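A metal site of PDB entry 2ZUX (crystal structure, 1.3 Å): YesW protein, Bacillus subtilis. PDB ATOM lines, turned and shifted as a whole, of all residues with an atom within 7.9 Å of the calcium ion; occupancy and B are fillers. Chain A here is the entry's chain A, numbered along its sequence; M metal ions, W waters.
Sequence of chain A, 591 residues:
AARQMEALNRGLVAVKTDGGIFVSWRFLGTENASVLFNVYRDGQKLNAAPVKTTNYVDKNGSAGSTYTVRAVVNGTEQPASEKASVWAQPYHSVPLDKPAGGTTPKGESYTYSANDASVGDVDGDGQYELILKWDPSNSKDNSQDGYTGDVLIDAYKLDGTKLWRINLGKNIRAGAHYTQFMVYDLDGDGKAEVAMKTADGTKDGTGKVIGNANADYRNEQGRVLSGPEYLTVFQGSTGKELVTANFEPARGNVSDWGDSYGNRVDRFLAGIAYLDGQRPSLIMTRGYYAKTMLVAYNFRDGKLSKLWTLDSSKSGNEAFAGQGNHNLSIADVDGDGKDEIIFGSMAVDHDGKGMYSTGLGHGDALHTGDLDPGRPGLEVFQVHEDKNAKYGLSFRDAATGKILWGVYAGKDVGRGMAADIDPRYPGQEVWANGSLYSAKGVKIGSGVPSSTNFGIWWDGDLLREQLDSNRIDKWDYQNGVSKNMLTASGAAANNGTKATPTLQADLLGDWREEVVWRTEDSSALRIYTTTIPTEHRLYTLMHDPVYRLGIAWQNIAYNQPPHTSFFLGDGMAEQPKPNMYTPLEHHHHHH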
ATOM      1  N   ASP A 420      13.318 -14.325  28.189  1.00  0.00           N
ATOM      2  CA  ASP A 420      12.492 -13.456  27.360  1.00  0.00           C
ATOM      3  C   ASP A 420      11.319 -12.977  28.204  1.00  0.00           C
ATOM      4  O   ASP A 420      10.350 -13.710  28.405  1.00  0.00           O
ATOM      5  CB  ASP A 420      11.976 -14.184  26.119  1.00  0.00           C
ATOM      6  CG  ASP A 420      11.271 -13.242  25.153  1.00  0.00           C
ATOM      7  OD1 ASP A 420      11.275 -12.015  25.408  1.00  0.00           O
ATOM      8  OD2 ASP A 420      10.721 -13.718  24.132  1.00  0.00           O
ATOM      9  N   ILE A 456      11.197 -19.497  34.673  1.00  0.00           N
ATOM     10  CA  ILE A 456      10.328 -20.664  34.518  1.00  0.00           C
ATOM     11  C   ILE A 456       9.220 -20.401  33.500  1.00  0.00           C
ATOM     12  O   ILE A 456       8.610 -19.315  33.505  1.00  0.00           O
ATOM     13  CB  ILE A 456       9.712 -21.070  35.881  1.00  0.00           C
ATOM     14  CG1 ILE A 456       8.914 -22.369  35.729  1.00  0.00           C
ATOM     15  CG2 ILE A 456       8.853 -19.930  36.466  1.00  0.00           C
ATOM     16  CD1 ILE A 456       8.393 -22.926  37.030  1.00  0.00           C
ATOM     17  N   TRP A 457       8.939 -21.376  32.640  1.00  0.00           N
ATOM     18  CA  TRP A 457       7.755 -21.306  31.770  1.00  0.00           C
ATOM     19  C   TRP A 457       6.571 -21.847  32.538  1.00  0.00           C
ATOM     20  O   TRP A 457       6.474 -23.048  32.766  1.00  0.00           O
ATOM     21  CB  TRP A 457       7.969 -22.070  30.454  1.00  0.00           C
ATOM     22  CG  TRP A 457       8.990 -21.393  29.577  1.00  0.00           C
ATOM     23  CD1 TRP A 457       8.848 -20.171  28.962  1.00  0.00           C
ATOM     24  CD2 TRP A 457      10.295 -21.872  29.234  1.00  0.00           C
ATOM     25  NE1 TRP A 457      10.000 -19.860  28.264  1.00  0.00           N
ATOM     26  CE2 TRP A 457      10.904 -20.878  28.420  1.00  0.00           C
ATOM     27  CE3 TRP A 457      11.025 -23.028  29.550  1.00  0.00           C
ATOM     28  CZ2 TRP A 457      12.190 -21.026  27.906  1.00  0.00           C
ATOM     29  CZ3 TRP A 457      12.315 -23.171  29.028  1.00  0.00           C
ATOM     30  CH2 TRP A 457      12.885 -22.161  28.231  1.00  0.00           C
ATOM     31  N   TRP A 458       5.687 -20.937  32.964  1.00  0.00           N
ATOM     32  CA  TRP A 458       4.575 -21.300  33.854  1.00  0.00           C
ATOM     33  C   TRP A 458       3.193 -20.995  33.306  1.00  0.00           C
ATOM     34  O   TRP A 458       2.292 -21.831  33.422  1.00  0.00           O
ATOM     35  CB  TRP A 458       4.754 -20.611  35.213  1.00  0.00           C
ATOM     36  CG  TRP A 458       3.701 -21.000  36.194  1.00  0.00           C
ATOM     37  CD1 TRP A 458       2.669 -20.223  36.642  1.00  0.00           C
ATOM     38  CD2 TRP A 458       3.564 -22.264  36.850  1.00  0.00           C
ATOM     39  NE1 TRP A 458       1.912 -20.927  37.554  1.00  0.00           N
ATOM     40  CE2 TRP A 458       2.435 -22.188  37.690  1.00  0.00           C
ATOM     41  CE3 TRP A 458       4.300 -23.464  36.820  1.00  0.00           C
ATOM     42  CZ2 TRP A 458       2.021 -23.259  38.499  1.00  0.00           C
ATOM     43  CZ3 TRP A 458       3.881 -24.524  37.622  1.00  0.00           C
ATOM     44  CH2 TRP A 458       2.750 -24.403  38.438  1.00  0.00           C
ATOM     45  N   ASP A 459       3.004 -19.801  32.740  1.00  0.00           N
ATOM     46  CA  ASP A 459       1.702 -19.460  32.189  1.00  0.00           C
ATOM     47  C   ASP A 459       1.592 -19.906  30.736  1.00  0.00           C
ATOM     48  O   ASP A 459       2.379 -20.726  30.256  1.00  0.00           O
ATOM     49  CB  ASP A 459       1.365 -17.970  32.406  1.00  0.00           C
ATOM     50  CG  ASP A 459       2.228 -17.029  31.581  1.00  0.00           C
ATOM     51  OD1 ASP A 459       2.884 -17.472  30.608  1.00  0.00           O
ATOM     52  OD2 ASP A 459       2.224 -15.831  31.917  1.00  0.00           O
ATOM     53  N   GLY A 460       0.595 -19.377  30.032  1.00  0.00           N
ATOM     54  CA  GLY A 460       0.327 -19.845  28.679  1.00  0.00           C
ATOM     55  C   GLY A 460       1.091 -19.157  27.568  1.00  0.00           C
ATOM     56  O   GLY A 460       1.057 -19.630  26.430  1.00  0.00           O
ATOM     57  N   ASP A 461       1.779 -18.059  27.872  1.00  0.00           N
ATOM     58  CA  ASP A 461       2.492 -17.340  26.820  1.00  0.00           C
ATOM     59  C   ASP A 461       3.943 -17.790  26.682  1.00  0.00           C
ATOM     60  O   ASP A 461       4.478 -18.478  27.559  1.00  0.00           O
ATOM     61  CB  ASP A 461       2.335 -15.816  26.954  1.00  0.00           C
ATOM     62  CG  ASP A 461       3.217 -15.206  28.043  1.00  0.00           C
ATOM     63  OD1 ASP A 461       4.226 -15.820  28.482  1.00  0.00           O
ATOM     64  OD2 ASP A 461       2.911 -14.063  28.452  1.00  0.00           O
ATOM     65  N   LEU A 462       4.565 -17.417  25.570  1.00  0.00           N
ATOM     66  CA  LEU A 462       5.920 -17.850  25.254  1.00  0.00           C
ATOM     67  C   LEU A 462       7.000 -17.048  25.986  1.00  0.00           C
ATOM     68  O   LEU A 462       8.171 -17.432  25.932  1.00  0.00           O
ATOM     69  CB  LEU A 462       6.139 -17.813  23.731  1.00  0.00           C
ATOM     70  CG  LEU A 462       5.278 -18.787  22.908  1.00  0.00           C
ATOM     71  CD1 LEU A 462       5.445 -18.482  21.427  1.00  0.00           C
ATOM     72  CD2 LEU A 462       5.640 -20.234  23.206  1.00  0.00           C
ATOM     73  N   LEU A 463       6.621 -15.990  26.677  1.00  0.00           N
ATOM     74  CA  LEU A 463       7.557 -15.289  27.557  1.00  0.00           C
ATOM     75  C   LEU A 463       7.865 -16.187  28.753  1.00  0.00           C
ATOM     76  O   LEU A 463       7.084 -17.104  29.057  1.00  0.00           O
ATOM     77  CB  LEU A 463       6.975 -13.948  28.033  1.00  0.00           C
ATOM     78  CG  LEU A 463       6.639 -12.930  26.937  1.00  0.00           C
ATOM     79  CD1 LEU A 463       6.003 -11.709  27.554  1.00  0.00           C
ATOM     80  CD2 LEU A 463       7.878 -12.541  26.126  1.00  0.00           C
ATOM     81  N   ARG A 464       8.991 -15.956  29.414  1.00  0.00           N
ATOM     82  CA  ARG A 464       9.345 -16.750  30.571  1.00  0.00           C
ATOM     83  C   ARG A 464       9.058 -15.978  31.843  1.00  0.00           C
ATOM     84  O   ARG A 464       9.346 -14.778  31.940  1.00  0.00           O
ATOM     85  CB  ARG A 464      10.804 -17.207  30.497  1.00  0.00           C
ATOM     86  CG  ARG A 464      11.073 -18.471  31.288  1.00  0.00           C
ATOM     87  CD  ARG A 464      12.417 -19.077  30.986  1.00  0.00           C
ATOM     88  NE  ARG A 464      12.521 -20.435  31.521  1.00  0.00           N
ATOM     89  CZ  ARG A 464      13.653 -21.125  31.613  1.00  0.00           C
ATOM     90  NH1 ARG A 464      14.805 -20.588  31.212  1.00  0.00           N
ATOM     91  NH2 ARG A 464      13.641 -22.357  32.107  1.00  0.00           N
ATOM     92  N   GLU A 465       8.486 -16.679  32.811  1.00  0.00           N
ATOM     93  CA  GLU A 465       8.183 -16.118  34.121  1.00  0.00           C
ATOM     94  C   GLU A 465       9.405 -16.269  35.036  1.00  0.00           C
ATOM     95  O   GLU A 465      10.439 -16.776  34.618  1.00  0.00           O
ATOM     96  CB  GLU A 465       6.925 -16.774  34.690  1.00  0.00           C
ATOM     97  CG  GLU A 465       5.613 -16.407  33.946  1.00  0.00           C
ATOM     98  CD  GLU A 465       5.558 -16.880  32.490  1.00  0.00           C
ATOM     99  OE1 GLU A 465       5.442 -18.102  32.259  1.00  0.00           O
ATOM    100  OE2 GLU A 465       5.606 -16.031  31.565  1.00  0.00           O
ATOM    101  N   LYS A 474       5.520 -12.747  37.417  1.00  0.00           N
ATOM    102  CA  LYS A 474       5.566 -12.357  36.020  1.00  0.00           C
ATOM    103  C   LYS A 474       5.931 -10.881  35.905  1.00  0.00           C
ATOM    104  O   LYS A 474       5.459 -10.048  36.677  1.00  0.00           O
ATOM    105  CB  LYS A 474       4.235 -12.630  35.308  1.00  0.00           C
ATOM    106  CG  LYS A 474       4.379 -12.588  33.777  1.00  0.00           C
ATOM    107  CD  LYS A 474       3.066 -12.856  33.078  1.00  0.00           C
ATOM    108  CE  LYS A 474       3.231 -12.696  31.594  1.00  0.00           C
ATOM    109  NZ  LYS A 474       4.013 -13.804  30.992  1.00  0.00           N
ATOM    110  N   MET A 485       2.355 -14.421  40.622  1.00  0.00           N
ATOM    111  CA  MET A 485       1.421 -15.332  39.956  1.00  0.00           C
ATOM    112  C   MET A 485       1.049 -16.497  40.868  1.00  0.00           C
ATOM    113  O   MET A 485      -0.084 -16.980  40.851  1.00  0.00           O
ATOM    114  CB  MET A 485       2.026 -15.905  38.684  1.00  0.00           C
ATOM    115  CG  MET A 485       2.137 -14.955  37.533  1.00  0.00           C
ATOM    116  SD  MET A 485       2.185 -15.883  35.994  1.00  0.00           S
ATOM    117  CE  MET A 485       0.433 -16.132  35.680  1.00  0.00           C
ATOM    118  N   TRP A 511       4.437 -28.641  27.880  1.00  0.00           N
ATOM    119  CA  TRP A 511       5.774 -28.051  27.886  1.00  0.00           C
ATOM    120  C   TRP A 511       6.106 -27.119  29.051  1.00  0.00           C
ATOM    121  O   TRP A 511       7.279 -26.832  29.270  1.00  0.00           O
ATOM    122  CB  TRP A 511       6.030 -27.327  26.560  1.00  0.00           C
ATOM    123  CG  TRP A 511       5.140 -26.149  26.320  1.00  0.00           C
ATOM    124  CD1 TRP A 511       3.874 -26.175  25.785  1.00  0.00           C
ATOM    125  CD2 TRP A 511       5.426 -24.767  26.582  1.00  0.00           C
ATOM    126  NE1 TRP A 511       3.366 -24.899  25.718  1.00  0.00           N
ATOM    127  CE2 TRP A 511       4.296 -24.018  26.208  1.00  0.00           C
ATOM    128  CE3 TRP A 511       6.538 -24.092  27.121  1.00  0.00           C
ATOM    129  CZ2 TRP A 511       4.239 -22.624  26.321  1.00  0.00           C
ATOM    130  CZ3 TRP A 511       6.481 -22.698  27.234  1.00  0.00           C
ATOM    131  CH2 TRP A 511       5.342 -21.991  26.842  1.00  0.00           C
ATOM    132  N   ARG A 512       5.096 -26.658  29.797  1.00  0.00           N
ATOM    133  CA  ARG A 512       5.416 -25.804  30.932  1.00  0.00           C
ATOM    134  C   ARG A 512       6.180 -26.598  31.996  1.00  0.00           C
ATOM    135  O   ARG A 512       6.085 -27.822  32.069  1.00  0.00           O
ATOM    136  CB  ARG A 512       4.169 -25.137  31.513  1.00  0.00           C
ATOM    137  CG  ARG A 512       3.767 -23.835  30.809  1.00  0.00           C
ATOM    138  CD  ARG A 512       3.085 -24.067  29.455  1.00  0.00           C
ATOM    139  NE  ARG A 512       1.860 -24.854  29.546  1.00  0.00           N
ATOM    140  CZ  ARG A 512       0.681 -24.381  29.921  1.00  0.00           C
ATOM    141  NH1 ARG A 512      -0.373 -25.196  29.964  1.00  0.00           N
ATOM    142  NH2 ARG A 512       0.531 -23.109  30.272  1.00  0.00           N
ATOM    143  N   THR A 534      -2.843 -23.010  27.549  1.00  0.00           N
ATOM    144  CA  THR A 534      -1.972 -22.462  26.517  1.00  0.00           C
ATOM    145  C   THR A 534      -2.481 -22.812  25.134  1.00  0.00           C
ATOM    146  O   THR A 534      -3.072 -23.874  24.926  1.00  0.00           O
ATOM    147  CB  THR A 534      -0.499 -22.912  26.697  1.00  0.00           C
ATOM    148  OG1 THR A 534       0.321 -22.240  25.732  1.00  0.00           O
ATOM    149  CG2 THR A 534      -0.340 -24.416  26.526  1.00  0.00           C
ATOM    150  N   HIS A 536      -0.218 -23.029  22.825  1.00  0.00           N
ATOM    151  CA  HIS A 536       1.035 -23.499  22.243  1.00  0.00           C
ATOM    152  C   HIS A 536       1.358 -24.933  22.594  1.00  0.00           C
ATOM    153  O   HIS A 536       1.216 -25.352  23.746  1.00  0.00           O
ATOM    154  CB  HIS A 536       2.207 -22.621  22.684  1.00  0.00           C
ATOM    155  CG  HIS A 536       2.029 -21.185  22.342  1.00  0.00           C
ATOM    156  ND1 HIS A 536       2.135 -20.710  21.054  1.00  0.00           N
ATOM    157  CD2 HIS A 536       1.735 -20.119  23.118  1.00  0.00           C
ATOM    158  CE1 HIS A 536       1.917 -19.413  21.053  1.00  0.00           C
ATOM    159  NE2 HIS A 536       1.666 -19.023  22.293  1.00  0.00           N
ATOM    160  N   LEU A 568      13.182 -20.226  22.668  1.00  0.00           N
ATOM    161  CA  LEU A 568      11.783 -20.401  23.038  1.00  0.00           C
ATOM    162  C   LEU A 568      11.343 -19.064  23.594  1.00  0.00           C
ATOM    163  O   LEU A 568      11.785 -18.641  24.657  1.00  0.00           O
ATOM    164  CB  LEU A 568      11.645 -21.507  24.088  1.00  0.00           C
ATOM    165  CG  LEU A 568      10.253 -22.109  24.330  1.00  0.00           C
ATOM    166  CD1 LEU A 568      10.363 -23.304  25.280  1.00  0.00           C
ATOM    167  CD2 LEU A 568       9.258 -21.086  24.864  1.00  0.00           C
HETATM  168 CA    CA M   1       4.997 -17.610  29.801  1.00  0.00          CA
HETATM  169  O   HOH W   1       5.077 -20.069  29.818  1.00  0.00           O
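The side-chain carboxylate (OD2) of Asp 461 is in salt-bridge range of the side-chain amino group (NZ) of Lys 474, at 2.8 Å.
The side-chain carboxylate of Glu 465 lies close to the side-chain amino group of Lys 474 (2.8 Å).
The backbone carbonyl oxygen (O) of Asp 459 is in hydrogen-bond range of the guanidinium group (NH2) of Arg 512 (3.0 Å).
OE1 of Glu 465 sits close to N of Trp 458, 2.9 Å away.
OD2 of Asp 459 lies within salt-bridge range of NZ of Lys 474 (2.9 Å).
O of Ile 456 sits at hydrogen-bond distance from N of Glu 465 (2.7 Å).
Of the 18 residues printed, 4 come within 4 Å of the calcium ion.
Along chain A the residues within 4 Å of the calcium ion span positions 459 to 465.
The side-chain carboxylate (OD1) of Asp 459 binds the calcium ion (2.3 Å).
The calcium ion is bound by the backbone carbonyl oxygen (O) of Leu 463 (2.3 Å).
The calcium ion is bound by the side-chain carboxylate (OD1) of Asp 461 (2.4 Å).
The calcium ion is bound by OE2 of Glu 465 (2.4 Å).
The calcium ion is bound by O of Asp 461, 2.5 Å away.
The calcium ion is bound by water W1, 2.5 Å away.
The side-chain carboxylate (OE1) of Glu 465 is bound to the calcium ion, at 2.5 Å.
The calcium ion has seven donor atoms within binding distance.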
